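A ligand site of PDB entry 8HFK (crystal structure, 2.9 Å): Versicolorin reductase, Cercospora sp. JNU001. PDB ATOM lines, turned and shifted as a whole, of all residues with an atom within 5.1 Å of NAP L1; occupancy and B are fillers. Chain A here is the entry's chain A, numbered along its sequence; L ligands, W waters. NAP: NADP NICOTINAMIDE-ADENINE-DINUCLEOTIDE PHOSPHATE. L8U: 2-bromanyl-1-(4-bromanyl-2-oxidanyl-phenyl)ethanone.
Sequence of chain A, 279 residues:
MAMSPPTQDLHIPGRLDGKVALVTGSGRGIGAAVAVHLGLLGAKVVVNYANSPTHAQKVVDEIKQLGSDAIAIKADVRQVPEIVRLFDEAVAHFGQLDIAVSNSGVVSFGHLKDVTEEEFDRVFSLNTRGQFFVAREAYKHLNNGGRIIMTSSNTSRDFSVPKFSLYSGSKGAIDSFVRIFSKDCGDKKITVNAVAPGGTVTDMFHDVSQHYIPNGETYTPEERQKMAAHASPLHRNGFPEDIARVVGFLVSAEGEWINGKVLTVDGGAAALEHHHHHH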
ATOM      1  N   THR A  24     -33.468 -27.906  12.642  1.00  0.00           N
ATOM      2  CA  THR A  24     -33.601 -28.060  11.164  1.00  0.00           C
ATOM      3  C   THR A  24     -32.269 -27.635  10.562  1.00  0.00           C
ATOM      4  O   THR A  24     -31.660 -26.668  11.074  1.00  0.00           O
ATOM      5  CB  THR A  24     -34.784 -27.289  10.567  1.00  0.00           C
ATOM      6  OG1 THR A  24     -34.502 -25.892  10.645  1.00  0.00           O
ATOM      7  CG2 THR A  24     -36.101 -27.630  11.237  1.00  0.00           C
ATOM      8  N   GLY A  25     -31.826 -28.364   9.543  1.00  0.00           N
ATOM      9  CA  GLY A  25     -30.543 -28.111   8.859  1.00  0.00           C
ATOM     10  C   GLY A  25     -29.367 -28.120   9.817  1.00  0.00           C
ATOM     11  O   GLY A  25     -28.494 -27.269   9.649  1.00  0.00           O
ATOM     12  N   SER A  26     -29.310 -29.060  10.762  1.00  0.00           N
ATOM     13  CA  SER A  26     -28.186 -29.172  11.730  1.00  0.00           C
ATOM     14  C   SER A  26     -27.089 -30.072  11.155  1.00  0.00           C
ATOM     15  O   SER A  26     -26.209 -30.527  11.908  1.00  0.00           O
ATOM     16  CB  SER A  26     -28.662 -29.622  13.110  1.00  0.00           C
ATOM     17  OG  SER A  26     -29.661 -30.628  13.039  1.00  0.00           O
ATOM     18  N   GLY A  27     -27.136 -30.306   9.835  1.00  0.00           N
ATOM     19  CA  GLY A  27     -26.074 -30.970   9.055  1.00  0.00           C
ATOM     20  C   GLY A  27     -24.808 -30.125   8.943  1.00  0.00           C
ATOM     21  O   GLY A  27     -23.724 -30.696   9.134  1.00  0.00           O
ATOM     22  N   ARG A  28     -24.926 -28.841   8.608  1.00  0.00           N
ATOM     23  CA  ARG A  28     -23.778 -27.923   8.363  1.00  0.00           C
ATOM     24  C   ARG A  28     -23.956 -26.598   9.093  1.00  0.00           C
ATOM     25  O   ARG A  28     -25.026 -26.370   9.724  1.00  0.00           O
ATOM     26  CB  ARG A  28     -23.671 -27.571   6.886  1.00  0.00           C
ATOM     27  CG  ARG A  28     -23.969 -28.743   5.961  1.00  0.00           C
ATOM     28  CD  ARG A  28     -23.784 -28.345   4.527  1.00  0.00           C
ATOM     29  NE  ARG A  28     -24.926 -27.598   4.010  1.00  0.00           N
ATOM     30  CZ  ARG A  28     -24.826 -26.485   3.313  1.00  0.00           C
ATOM     31  NH1 ARG A  28     -23.637 -25.960   3.054  1.00  0.00           N
ATOM     32  NH2 ARG A  28     -25.915 -25.894   2.861  1.00  0.00           N
ATOM     33  N   GLY A  29     -22.945 -25.737   8.972  1.00  0.00           N
ATOM     34  CA  GLY A  29     -22.989 -24.322   9.388  1.00  0.00           C
ATOM     35  C   GLY A  29     -23.452 -24.186  10.826  1.00  0.00           C
ATOM     36  O   GLY A  29     -23.086 -25.036  11.644  1.00  0.00           O
ATOM     37  N   ILE A  30     -24.283 -23.170  11.077  1.00  0.00           N
ATOM     38  CA  ILE A  30     -24.808 -22.763  12.413  1.00  0.00           C
ATOM     39  C   ILE A  30     -25.534 -23.955  13.034  1.00  0.00           C
ATOM     40  O   ILE A  30     -25.222 -24.305  14.196  1.00  0.00           O
ATOM     41  CB  ILE A  30     -25.700 -21.509  12.265  1.00  0.00           C
ATOM     42  CG1 ILE A  30     -24.950 -20.370  11.566  1.00  0.00           C
ATOM     43  CG2 ILE A  30     -26.279 -21.059  13.607  1.00  0.00           C
ATOM     44  CD1 ILE A  30     -25.811 -19.159  11.270  1.00  0.00           C
ATOM     45  N   GLY A  31     -26.458 -24.578  12.279  1.00  0.00           N
ATOM     46  CA  GLY A  31     -27.342 -25.648  12.792  1.00  0.00           C
ATOM     47  C   GLY A  31     -26.574 -26.752  13.511  1.00  0.00           C
ATOM     48  O   GLY A  31     -27.031 -27.219  14.573  1.00  0.00           O
ATOM     49  N   ASN A  48     -31.966 -32.868  11.945  1.00  0.00           N
ATOM     50  CA  ASN A  48     -32.645 -32.742  10.617  1.00  0.00           C
ATOM     51  C   ASN A  48     -31.644 -32.252   9.547  1.00  0.00           C
ATOM     52  O   ASN A  48     -30.656 -31.547   9.882  1.00  0.00           O
ATOM     53  CB  ASN A  48     -33.870 -31.831  10.723  1.00  0.00           C
ATOM     54  CG  ASN A  48     -34.520 -31.528   9.387  1.00  0.00           C
ATOM     55  OD1 ASN A  48     -34.431 -30.393   8.909  1.00  0.00           O
ATOM     56  ND2 ASN A  48     -35.147 -32.535   8.795  1.00  0.00           N
ATOM     57  N   TYR A  49     -31.911 -32.603   8.281  1.00  0.00           N
ATOM     58  CA  TYR A  49     -31.149 -32.235   7.064  1.00  0.00           C
ATOM     59  C   TYR A  49     -32.019 -32.588   5.850  1.00  0.00           C
ATOM     60  O   TYR A  49     -32.940 -33.433   6.007  1.00  0.00           O
ATOM     61  CB  TYR A  49     -29.801 -32.972   7.017  1.00  0.00           C
ATOM     62  CG  TYR A  49     -29.990 -34.451   6.765  1.00  0.00           C
ATOM     63  CD1 TYR A  49     -30.340 -35.301   7.801  1.00  0.00           C
ATOM     64  CD2 TYR A  49     -29.928 -34.983   5.486  1.00  0.00           C
ATOM     65  CE1 TYR A  49     -30.599 -36.640   7.586  1.00  0.00           C
ATOM     66  CE2 TYR A  49     -30.171 -36.320   5.259  1.00  0.00           C
ATOM     67  CZ  TYR A  49     -30.508 -37.155   6.315  1.00  0.00           C
ATOM     68  OH  TYR A  49     -30.773 -38.477   6.112  1.00  0.00           O
ATOM     69  N   ALA A  50     -31.735 -31.973   4.699  1.00  0.00           N
ATOM     70  CA  ALA A  50     -32.469 -32.273   3.455  1.00  0.00           C
ATOM     71  C   ALA A  50     -31.548 -32.921   2.422  1.00  0.00           C
ATOM     72  O   ALA A  50     -31.997 -33.842   1.748  1.00  0.00           O
ATOM     73  CB  ALA A  50     -33.048 -30.994   2.929  1.00  0.00           C
ATOM     74  N   ASN A  51     -30.288 -32.488   2.330  1.00  0.00           N
ATOM     75  CA  ASN A  51     -29.399 -32.973   1.241  1.00  0.00           C
ATOM     76  C   ASN A  51     -28.026 -33.401   1.760  1.00  0.00           C
ATOM     77  O   ASN A  51     -27.294 -34.006   0.983  1.00  0.00           O
ATOM     78  CB  ASN A  51     -29.212 -31.895   0.162  1.00  0.00           C
ATOM     79  CG  ASN A  51     -30.503 -31.235  -0.271  1.00  0.00           C
ATOM     80  OD1 ASN A  51     -30.824 -30.134   0.170  1.00  0.00           O
ATOM     81  ND2 ASN A  51     -31.235 -31.897  -1.149  1.00  0.00           N
ATOM     82  N   SER A  52     -27.714 -33.123   3.019  1.00  0.00           N
ATOM     83  CA  SER A  52     -26.362 -33.414   3.573  1.00  0.00           C
ATOM     84  C   SER A  52     -26.420 -34.530   4.612  1.00  0.00           C
ATOM     85  O   SER A  52     -26.129 -34.257   5.779  1.00  0.00           O
ATOM     86  CB  SER A  52     -25.773 -32.176   4.164  1.00  0.00           C
ATOM     87  OG  SER A  52     -25.490 -31.229   3.163  1.00  0.00           O
ATOM     88  N   ALA A  75     -35.616 -34.585   6.163  1.00  0.00           N
ATOM     89  CA  ALA A  75     -36.874 -33.893   5.794  1.00  0.00           C
ATOM     90  C   ALA A  75     -36.573 -32.565   5.104  1.00  0.00           C
ATOM     91  O   ALA A  75     -35.696 -31.826   5.598  1.00  0.00           O
ATOM     92  CB  ALA A  75     -37.735 -33.716   7.016  1.00  0.00           C
ATOM     93  N   ASP A  76     -37.281 -32.291   3.996  1.00  0.00           N
ATOM     94  CA  ASP A  76     -37.256 -30.997   3.260  1.00  0.00           C
ATOM     95  C   ASP A  76     -38.337 -30.113   3.883  1.00  0.00           C
ATOM     96  O   ASP A  76     -39.521 -30.476   3.745  1.00  0.00           O
ATOM     97  CB  ASP A  76     -37.499 -31.203   1.763  1.00  0.00           C
ATOM     98  CG  ASP A  76     -37.800 -29.932   0.985  1.00  0.00           C
ATOM     99  OD1 ASP A  76     -37.552 -28.827   1.525  1.00  0.00           O
ATOM    100  OD2 ASP A  76     -38.300 -30.051  -0.170  1.00  0.00           O
ATOM    101  N   VAL A  77     -37.944 -29.012   4.556  1.00  0.00           N
ATOM    102  CA  VAL A  77     -38.892 -28.210   5.378  1.00  0.00           C
ATOM    103  C   VAL A  77     -39.572 -27.200   4.458  1.00  0.00           C
ATOM    104  O   VAL A  77     -40.253 -26.315   5.000  1.00  0.00           O
ATOM    105  CB  VAL A  77     -38.277 -27.531   6.630  1.00  0.00           C
ATOM    106  CG1 VAL A  77     -37.452 -28.480   7.487  1.00  0.00           C
ATOM    107  CG2 VAL A  77     -37.460 -26.299   6.295  1.00  0.00           C
ATOM    108  N   ARG A  78     -39.404 -27.341   3.134  1.00  0.00           N
ATOM    109  CA  ARG A  78     -40.243 -26.683   2.087  1.00  0.00           C
ATOM    110  C   ARG A  78     -41.585 -27.412   1.950  1.00  0.00           C
ATOM    111  O   ARG A  78     -42.578 -26.696   1.742  1.00  0.00           O
ATOM    112  CB  ARG A  78     -39.557 -26.624   0.726  1.00  0.00           C
ATOM    113  CG  ARG A  78     -38.577 -25.473   0.578  1.00  0.00           C
ATOM    114  CD  ARG A  78     -38.162 -25.239  -0.875  1.00  0.00           C
ATOM    115  NE  ARG A  78     -37.290 -24.078  -1.077  1.00  0.00           N
ATOM    116  CZ  ARG A  78     -35.961 -24.070  -0.960  1.00  0.00           C
ATOM    117  NH1 ARG A  78     -35.277 -25.144  -0.633  1.00  0.00           N
ATOM    118  NH2 ARG A  78     -35.298 -22.946  -1.173  1.00  0.00           N
ATOM    119  N   ASN A 103     -33.729 -23.567  12.000  1.00  0.00           N
ATOM    120  CA  ASN A 103     -32.410 -23.007  11.588  1.00  0.00           C
ATOM    121  C   ASN A 103     -32.256 -22.922  10.051  1.00  0.00           C
ATOM    122  O   ASN A 103     -31.551 -22.001   9.589  1.00  0.00           O
ATOM    123  CB  ASN A 103     -31.228 -23.788  12.182  1.00  0.00           C
ATOM    124  CG  ASN A 103     -29.917 -23.434  11.507  1.00  0.00           C
ATOM    125  OD1 ASN A 103     -29.374 -22.336  11.672  1.00  0.00           O
ATOM    126  ND2 ASN A 103     -29.427 -24.356  10.684  1.00  0.00           N
ATOM    127  N   SER A 104     -32.868 -23.834   9.303  1.00  0.00           N
ATOM    128  CA  SER A 104     -32.688 -23.986   7.830  1.00  0.00           C
ATOM    129  C   SER A 104     -32.975 -22.681   7.077  1.00  0.00           C
ATOM    130  O   SER A 104     -34.048 -22.059   7.299  1.00  0.00           O
ATOM    131  CB  SER A 104     -33.573 -25.113   7.310  1.00  0.00           C
ATOM    132  OG  SER A 104     -33.201 -26.366   7.858  1.00  0.00           O
ATOM    133  N   GLY A 105     -32.101 -22.311   6.131  1.00  0.00           N
ATOM    134  CA  GLY A 105     -32.332 -21.136   5.275  1.00  0.00           C
ATOM    135  C   GLY A 105     -31.369 -21.043   4.108  1.00  0.00           C
ATOM    136  O   GLY A 105     -30.314 -21.729   4.125  1.00  0.00           O
ATOM    137  N   VAL A 106     -31.701 -20.194   3.138  1.00  0.00           N
ATOM    138  CA  VAL A 106     -30.877 -19.926   1.930  1.00  0.00           C
ATOM    139  C   VAL A 106     -30.699 -18.406   1.773  1.00  0.00           C
ATOM    140  O   VAL A 106     -31.505 -17.623   2.332  1.00  0.00           O
ATOM    141  CB  VAL A 106     -31.533 -20.576   0.696  1.00  0.00           C
ATOM    142  CG1 VAL A 106     -31.464 -22.087   0.809  1.00  0.00           C
ATOM    143  CG2 VAL A 106     -32.969 -20.122   0.508  1.00  0.00           C
ATOM    144  N   LEU A 126     -38.795 -21.798   2.022  1.00  0.00           N
ATOM    145  CA  LEU A 126     -37.893 -22.396   3.063  1.00  0.00           C
ATOM    146  C   LEU A 126     -37.761 -21.421   4.240  1.00  0.00           C
ATOM    147  O   LEU A 126     -37.927 -21.862   5.414  1.00  0.00           O
ATOM    148  CB  LEU A 126     -36.507 -22.705   2.474  1.00  0.00           C
ATOM    149  CG  LEU A 126     -35.462 -23.255   3.462  1.00  0.00           C
ATOM    150  CD1 LEU A 126     -35.816 -24.661   3.956  1.00  0.00           C
ATOM    151  CD2 LEU A 126     -34.070 -23.265   2.844  1.00  0.00           C
ATOM    152  N   ASN A 127     -37.443 -20.162   3.946  1.00  0.00           N
ATOM    153  CA  ASN A 127     -36.967 -19.176   4.943  1.00  0.00           C
ATOM    154  C   ASN A 127     -38.129 -18.695   5.802  1.00  0.00           C
ATOM    155  O   ASN A 127     -37.885 -18.439   7.002  1.00  0.00           O
ATOM    156  CB  ASN A 127     -36.302 -17.964   4.297  1.00  0.00           C
ATOM    157  CG  ASN A 127     -34.950 -18.268   3.699  1.00  0.00           C
ATOM    158  OD1 ASN A 127     -34.597 -19.426   3.496  1.00  0.00           O
ATOM    159  ND2 ASN A 127     -34.209 -17.214   3.424  1.00  0.00           N
ATOM    160  N   THR A 151     -34.613 -18.645  13.239  1.00  0.00           N
ATOM    161  CA  THR A 151     -33.407 -17.884  12.840  1.00  0.00           C
ATOM    162  C   THR A 151     -33.858 -16.763  11.923  1.00  0.00           C
ATOM    163  O   THR A 151     -34.664 -17.052  11.028  1.00  0.00           O
ATOM    164  CB  THR A 151     -32.330 -18.759  12.181  1.00  0.00           C
ATOM    165  OG1 THR A 151     -32.177 -19.984  12.897  1.00  0.00           O
ATOM    166  CG2 THR A 151     -31.003 -18.045  12.151  1.00  0.00           C
ATOM    167  N   SER A 152     -33.422 -15.536  12.208  1.00  0.00           N
ATOM    168  CA  SER A 152     -33.653 -14.305  11.411  1.00  0.00           C
ATOM    169  C   SER A 152     -32.319 -13.850  10.817  1.00  0.00           C
ATOM    170  O   SER A 152     -31.510 -14.720  10.456  1.00  0.00           O
ATOM    171  CB  SER A 152     -34.286 -13.262  12.274  1.00  0.00           C
ATOM    172  OG  SER A 152     -34.670 -12.134  11.507  1.00  0.00           O
ATOM    173  N   SER A 153     -32.077 -12.544  10.778  1.00  0.00           N
ATOM    174  CA  SER A 153     -30.864 -11.931  10.163  1.00  0.00           C
ATOM    175  C   SER A 153     -30.705 -10.511  10.705  1.00  0.00           C
ATOM    176  O   SER A 153     -31.731  -9.942  11.072  1.00  0.00           O
ATOM    177  CB  SER A 153     -31.022 -11.983   8.658  1.00  0.00           C
ATOM    178  OG  SER A 153     -30.027 -11.211   7.996  1.00  0.00           O
ATOM    179  N   TYR A 167     -33.982 -11.841   0.339  1.00  0.00           N
ATOM    180  CA  TYR A 167     -33.444 -12.535   1.535  1.00  0.00           C
ATOM    181  C   TYR A 167     -33.969 -11.805   2.758  1.00  0.00           C
ATOM    182  O   TYR A 167     -34.720 -12.435   3.530  1.00  0.00           O
ATOM    183  CB  TYR A 167     -31.915 -12.560   1.620  1.00  0.00           C
ATOM    184  CG  TYR A 167     -31.383 -13.126   2.917  1.00  0.00           C
ATOM    185  CD1 TYR A 167     -31.464 -14.483   3.181  1.00  0.00           C
ATOM    186  CD2 TYR A 167     -30.834 -12.317   3.903  1.00  0.00           C
ATOM    187  CE1 TYR A 167     -30.976 -15.024   4.361  1.00  0.00           C
ATOM    188  CE2 TYR A 167     -30.359 -12.838   5.087  1.00  0.00           C
ATOM    189  CZ  TYR A 167     -30.438 -14.198   5.321  1.00  0.00           C
ATOM    190  OH  TYR A 167     -29.999 -14.728   6.507  1.00  0.00           O
ATOM    191  N   LYS A 171     -36.971 -12.816   6.144  1.00  0.00           N
ATOM    192  CA  LYS A 171     -36.554 -12.903   7.573  1.00  0.00           C
ATOM    193  C   LYS A 171     -37.300 -11.903   8.463  1.00  0.00           C
ATOM    194  O   LYS A 171     -37.592 -12.266   9.607  1.00  0.00           O
ATOM    195  CB  LYS A 171     -35.046 -12.662   7.639  1.00  0.00           C
ATOM    196  CG  LYS A 171     -34.228 -13.614   6.785  1.00  0.00           C
ATOM    197  CD  LYS A 171     -34.461 -15.032   7.185  1.00  0.00           C
ATOM    198  CE  LYS A 171     -33.179 -15.823   7.272  1.00  0.00           C
ATOM    199  NZ  LYS A 171     -33.350 -16.939   8.218  1.00  0.00           N
ATOM    200  N   PRO A 197     -28.594 -13.737  13.448  1.00  0.00           N
ATOM    201  CA  PRO A 197     -27.181 -13.822  13.247  1.00  0.00           C
ATOM    202  C   PRO A 197     -26.663 -12.744  12.291  1.00  0.00           C
ATOM    203  O   PRO A 197     -27.424 -12.229  11.523  1.00  0.00           O
ATOM    204  CB  PRO A 197     -27.019 -15.222  12.641  1.00  0.00           C
ATOM    205  CG  PRO A 197     -28.198 -15.981  13.140  1.00  0.00           C
ATOM    206  CD  PRO A 197     -29.283 -14.941  12.980  1.00  0.00           C
ATOM    207  N   GLY A 198     -25.364 -12.442  12.367  1.00  0.00           N
ATOM    208  CA  GLY A 198     -24.751 -11.431  11.484  1.00  0.00           C
ATOM    209  C   GLY A 198     -24.077 -12.068  10.273  1.00  0.00           C
ATOM    210  O   GLY A 198     -24.772 -12.297   9.288  1.00  0.00           O
ATOM    211  N   GLY A 199     -22.775 -12.332  10.364  1.00  0.00           N
ATOM    212  CA  GLY A 199     -22.019 -12.923   9.233  1.00  0.00           C
ATOM    213  C   GLY A 199     -21.241 -14.151   9.647  1.00  0.00           C
ATOM    214  O   GLY A 199     -20.082 -14.283   9.214  1.00  0.00           O
ATOM    215  N   THR A 200     -21.857 -15.023  10.441  1.00  0.00           N
ATOM    216  CA  THR A 200     -21.171 -16.248  10.935  1.00  0.00           C
ATOM    217  C   THR A 200     -20.472 -16.962   9.771  1.00  0.00           C
ATOM    218  O   THR A 200     -21.164 -17.270   8.773  1.00  0.00           O
ATOM    219  CB  THR A 200     -22.163 -17.175  11.666  1.00  0.00           C
ATOM    220  OG1 THR A 200     -22.069 -18.480  11.109  1.00  0.00           O
ATOM    221  CG2 THR A 200     -23.588 -16.673  11.567  1.00  0.00           C
ATOM    222  N   THR A 202     -19.608 -19.316   7.260  1.00  0.00           N
ATOM    223  CA  THR A 202     -20.265 -20.531   6.748  1.00  0.00           C
ATOM    224  C   THR A 202     -20.149 -20.478   5.221  1.00  0.00           C
ATOM    225  O   THR A 202     -19.690 -19.443   4.734  1.00  0.00           O
ATOM    226  CB  THR A 202     -21.743 -20.600   7.144  1.00  0.00           C
ATOM    227  OG1 THR A 202     -22.391 -19.431   6.654  1.00  0.00           O
ATOM    228  CG2 THR A 202     -21.962 -20.732   8.639  1.00  0.00           C
ATOM    229  N   ASP A 203     -20.550 -21.538   4.515  1.00  0.00           N
ATOM    230  CA  ASP A 203     -20.573 -21.496   3.020  1.00  0.00           C
ATOM    231  C   ASP A 203     -21.505 -20.373   2.568  1.00  0.00           C
ATOM    232  O   ASP A 203     -21.255 -19.839   1.488  1.00  0.00           O
ATOM    233  CB  ASP A 203     -20.890 -22.879   2.449  1.00  0.00           C
ATOM    234  CG  ASP A 203     -19.727 -23.837   2.448  1.00  0.00           C
ATOM    235  OD1 ASP A 203     -18.635 -23.432   2.868  1.00  0.00           O
ATOM    236  OD2 ASP A 203     -19.932 -24.979   2.035  1.00  0.00           O
ATOM    237  N   MET A 204     -22.492 -19.974   3.387  1.00  0.00           N
ATOM    238  CA  MET A 204     -23.437 -18.885   3.057  1.00  0.00           C
ATOM    239  C   MET A 204     -22.767 -17.524   3.226  1.00  0.00           C
ATOM    240  O   MET A 204     -22.909 -16.706   2.328  1.00  0.00           O
ATOM    241  CB  MET A 204     -24.667 -18.942   3.961  1.00  0.00           C
ATOM    242  CG  MET A 204     -25.920 -18.376   3.331  1.00  0.00           C
ATOM    243  SD  MET A 204     -27.188 -17.879   4.529  1.00  0.00           S
ATOM    244  CE  MET A 204     -28.168 -19.374   4.606  1.00  0.00           C
ATOM    245  N   PHE A 205     -22.047 -17.306   4.321  1.00  0.00           N
ATOM    246  CA  PHE A 205     -21.265 -16.057   4.494  1.00  0.00           C
ATOM    247  C   PHE A 205     -20.316 -15.861   3.332  1.00  0.00           C
ATOM    248  O   PHE A 205     -20.195 -14.720   2.829  1.00  0.00           O
ATOM    249  CB  PHE A 205     -20.389 -16.120   5.743  1.00  0.00           C
ATOM    250  CG  PHE A 205     -19.450 -14.962   5.916  1.00  0.00           C
ATOM    251  CD1 PHE A 205     -19.931 -13.689   6.143  1.00  0.00           C
ATOM    252  CD2 PHE A 205     -18.086 -15.147   5.859  1.00  0.00           C
ATOM    253  CE1 PHE A 205     -19.070 -12.626   6.296  1.00  0.00           C
ATOM    254  CE2 PHE A 205     -17.210 -14.085   6.014  1.00  0.00           C
ATOM    255  CZ  PHE A 205     -17.706 -12.820   6.237  1.00  0.00           C
HETATM  256  PA  NAP L   1     -25.633 -22.892   5.393  1.00  0.00           P
HETATM  257  O1A NAP L   1     -24.302 -23.331   5.662  1.00  0.00           O
HETATM  258  O2A NAP L   1     -26.067 -22.627   4.077  1.00  0.00           O
HETATM  259  O5B NAP L   1     -26.478 -24.007   5.912  1.00  0.00           O
HETATM  260  C5B NAP L   1     -27.722 -24.231   5.356  1.00  0.00           C
HETATM  261  C4B NAP L   1     -28.525 -25.151   6.213  1.00  0.00           C
HETATM  262  O4B NAP L   1     -29.802 -25.063   5.663  1.00  0.00           O
HETATM  263  C3B NAP L   1     -28.099 -26.578   6.063  1.00  0.00           C
HETATM  264  O3B NAP L   1     -28.317 -27.318   7.239  1.00  0.00           O
HETATM  265  C2B NAP L   1     -29.054 -27.091   5.032  1.00  0.00           C
HETATM  266  O2B NAP L   1     -29.161 -28.511   5.041  1.00  0.00           O
HETATM  267  C1B NAP L   1     -30.274 -26.358   5.482  1.00  0.00           C
HETATM  268  N9A NAP L   1     -31.286 -26.490   4.474  1.00  0.00           N
HETATM  269  C8A NAP L   1     -31.343 -26.018   3.270  1.00  0.00           C
HETATM  270  N7A NAP L   1     -32.435 -26.409   2.611  1.00  0.00           N
HETATM  271  C5A NAP L   1     -33.102 -27.149   3.465  1.00  0.00           C
HETATM  272  C6A NAP L   1     -34.350 -27.883   3.477  1.00  0.00           C
HETATM  273  N6A NAP L   1     -35.184 -27.947   2.448  1.00  0.00           N
HETATM  274  N1A NAP L   1     -34.638 -28.513   4.571  1.00  0.00           N
HETATM  275  C2A NAP L   1     -33.860 -28.497   5.632  1.00  0.00           C
HETATM  276  N3A NAP L   1     -32.742 -27.864   5.712  1.00  0.00           N
HETATM  277  C4A NAP L   1     -32.335 -27.195   4.678  1.00  0.00           C
HETATM  278  O3  NAP L   1     -26.165 -21.656   6.179  1.00  0.00           O
HETATM  279  PN  NAP L   1     -25.953 -21.099   7.613  1.00  0.00           P
HETATM  280  O1N NAP L   1     -25.864 -22.140   8.577  1.00  0.00           O
HETATM  281  O2N NAP L   1     -24.911 -20.177   7.526  1.00  0.00           O
HETATM  282  O5D NAP L   1     -27.248 -20.351   7.874  1.00  0.00           O
HETATM  283  C5D NAP L   1     -27.962 -20.615   9.043  1.00  0.00           C
HETATM  284  C4D NAP L   1     -29.187 -19.782   9.247  1.00  0.00           C
HETATM  285  O4D NAP L   1     -28.814 -18.536   9.699  1.00  0.00           O
HETATM  286  C3D NAP L   1     -29.934 -19.503   8.011  1.00  0.00           C
HETATM  287  O3D NAP L   1     -31.216 -19.330   8.508  1.00  0.00           O
HETATM  288  C2D NAP L   1     -29.450 -18.177   7.517  1.00  0.00           C
HETATM  289  O2D NAP L   1     -30.393 -17.468   6.723  1.00  0.00           O
HETATM  290  C1D NAP L   1     -29.145 -17.490   8.805  1.00  0.00           C
HETATM  291  N1N NAP L   1     -28.060 -16.537   8.746  1.00  0.00           N
HETATM  292  C2N NAP L   1     -26.848 -16.913   8.474  1.00  0.00           C
HETATM  293  C3N NAP L   1     -25.855 -15.996   8.454  1.00  0.00           C
HETATM  294  C7N NAP L   1     -24.479 -16.324   8.125  1.00  0.00           C
HETATM  295  O7N NAP L   1     -23.734 -15.466   7.878  1.00  0.00           O
HETATM  296  N7N NAP L   1     -24.090 -17.539   8.117  1.00  0.00           N
HETATM  297  C4N NAP L   1     -26.132 -14.687   8.735  1.00  0.00           C
HETATM  298  C5N NAP L   1     -27.388 -14.325   9.029  1.00  0.00           C
HETATM  299  C6N NAP L   1     -28.327 -15.300   9.023  1.00  0.00           C
HETATM  300  P2B NAP L   1     -28.869 -29.345   3.793  1.00  0.00           P
HETATM  301  O1X NAP L   1     -29.669 -30.514   3.971  1.00  0.00           O
HETATM  302  O2X NAP L   1     -27.475 -29.665   3.843  1.00  0.00           O
HETATM  303  O3X NAP L   1     -29.292 -28.445   2.768  1.00  0.00           O
HETATM  304  C01 L8U L   2     -23.194 -10.705   6.679  1.00  0.00           C
HETATM  305  C02 L8U L   2     -23.676  -9.700   7.496  1.00  0.00           C
HETATM  306  C03 L8U L   2     -25.003  -9.594   7.793  1.00  0.00           C
HETATM  307  C04 L8U L   2     -25.880 -10.509   7.295  1.00  0.00           C
HETATM  308  C05 L8U L   2     -25.411 -11.504   6.480  1.00  0.00           C
HETATM  309  C06 L8U L   2     -24.076 -11.624   6.157  1.00  0.00           C
HETATM  310  C07 L8U L   2     -26.440 -12.476   5.957  1.00  0.00           C
HETATM  311  C08 L8U L   2     -26.311 -13.060   4.590  1.00  0.00           C
HETATM  312  O09 L8U L   2     -27.349 -12.804   6.609  1.00  0.00           O
HETATM  313  O10 L8U L   2     -27.231 -10.423   7.592  1.00  0.00           O
HETATM  314 BR1  L8U L   2     -26.873 -14.848   5.002  1.00  0.00          BR
HETATM  315 BR2  L8U L   2     -22.556  -8.361   8.290  1.00  0.00          BR
HETATM  316  O   HOH W   1     -28.523 -26.166   0.840  1.00  0.00           O
HETATM  317  O   HOH W   2     -32.962 -25.936   0.185  1.00  0.00           O
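O of Gly 25 is in hydrogen-bond range of O3B of NAP L1 (2.4 Å).
The backbone NH of Ser 52 sits at hydrogen-bond distance from an oxygen (O1X) of NAP L1, at 3.4 Å.
The side-chain hydroxyl (OG) of Ser 52 lies within hydrogen-bond range of an oxygen (O2X) of NAP L1 (2.6 Å).
O1X of NAP L1 sits at hydrogen-bond distance from N of Ala 50.
An oxygen (O1X) of NAP L1 is in hydrogen-bond range of the backbone NH of Asn 51, at 2.6 Å.
O3X of NAP L1 lies close to OD1 of Asn 51 (3.5 Å).
A nitrogen (N3A) of NAP L1 sits at hydrogen-bond distance from the side-chain hydroxyl (OG) of Ser 104.
N6A of NAP L1 sits at hydrogen-bond distance from OD1 of Asp 76 (2.7 Å).
An oxygen (O2N) of NAP L1 is in hydrogen-bond range of the side-chain hydroxyl (OG1) of Thr 202.
The side-chain hydroxyl (OH) of Tyr 167 lies within hydrogen-bond range of an oxygen (O2D) of NAP L1 (2.8 Å).
The backbone carbonyl oxygen (O) of Asn 103 is in hydrogen-bond range of an oxygen (O3D) of NAP L1 (2.9 Å).
N of Thr 200 is in hydrogen-bond range of O7N of NAP L1.
The backbone carbonyl oxygen of Thr 200 is in hydrogen-bond range of a nitrogen (N7N) of NAP L1.
N of Ile 30 is in hydrogen-bond range of O1N of NAP L1, at 3.1 Å.
The side-chain amino group (NZ) of Lys 171 is in hydrogen-bond range of an oxygen (O3D) of NAP L1.
The guanidinium group of Arg 28 lies within salt-bridge range of an oxygen (O2X) of NAP L1 (3.3 Å).
N1A of NAP L1 lies within hydrogen-bond range of N of Val 77 (3.3 Å).
The side-chain hydroxyl (OH) of Tyr 167 lies within hydrogen-bond range of an oxygen (O09) of L8U L2, 3.3 Å away.
An oxygen (O10) of L8U L2 sits at hydrogen-bond distance from the side-chain hydroxyl of Ser 153 (2.9 Å).
The side-chain amide oxygen of Asn 48 is in hydrogen-bond range of the backbone NH of Gly 25 (3.4 Å).
N of Ser 104 is in hydrogen-bond range of OG1 of Thr 24 (3.0 Å).
OG1 of Thr 202 sits at hydrogen-bond distance from O of Thr 200 (3.3 Å).
The side-chain hydroxyl (OG1) of Thr 202 sits close to the backbone NH (N) of Met 204, at 3.3 Å.
The side-chain amide nitrogen (ND2) of Asn 103 sits close to the backbone NH (N) of Gly 31 (3.4 Å).
N of Asn 103 sits at hydrogen-bond distance from OG1 of Thr 24 (2.8 Å).
O of Thr 151 lies within hydrogen-bond range of NZ of Lys 171, at 3.1 Å.
ND2 of Asn 48 is in hydrogen-bond range of O of Ala 75, at 3.3 Å.
Residues that only touch NAP L1: Gly 198 (2.8 Å), Pro 197 (3.3 Å), Thr 151 (3.3 Å), Gly 199 (3.3 Å), Met 204 (3.4 Å), Ser 152 (3.5 Å), Leu 126 (3.6 Å), Gly 105 (3.6 Å), Ala 75 (3.6 Å), Tyr 49 (3.7 Å), Gly 29 (3.7 Å) and Asn 48 (3.8 Å).
Water W2 bridges a nitrogen (N7A) of NAP L1 (2.5 Å) and the guanidinium group of Arg 78 (2.6 Å).
Water W1 lies within hydrogen-bond range of O3X of NAP L1 (3.1 Å) and NH2 of Arg 28 (3.3 Å).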
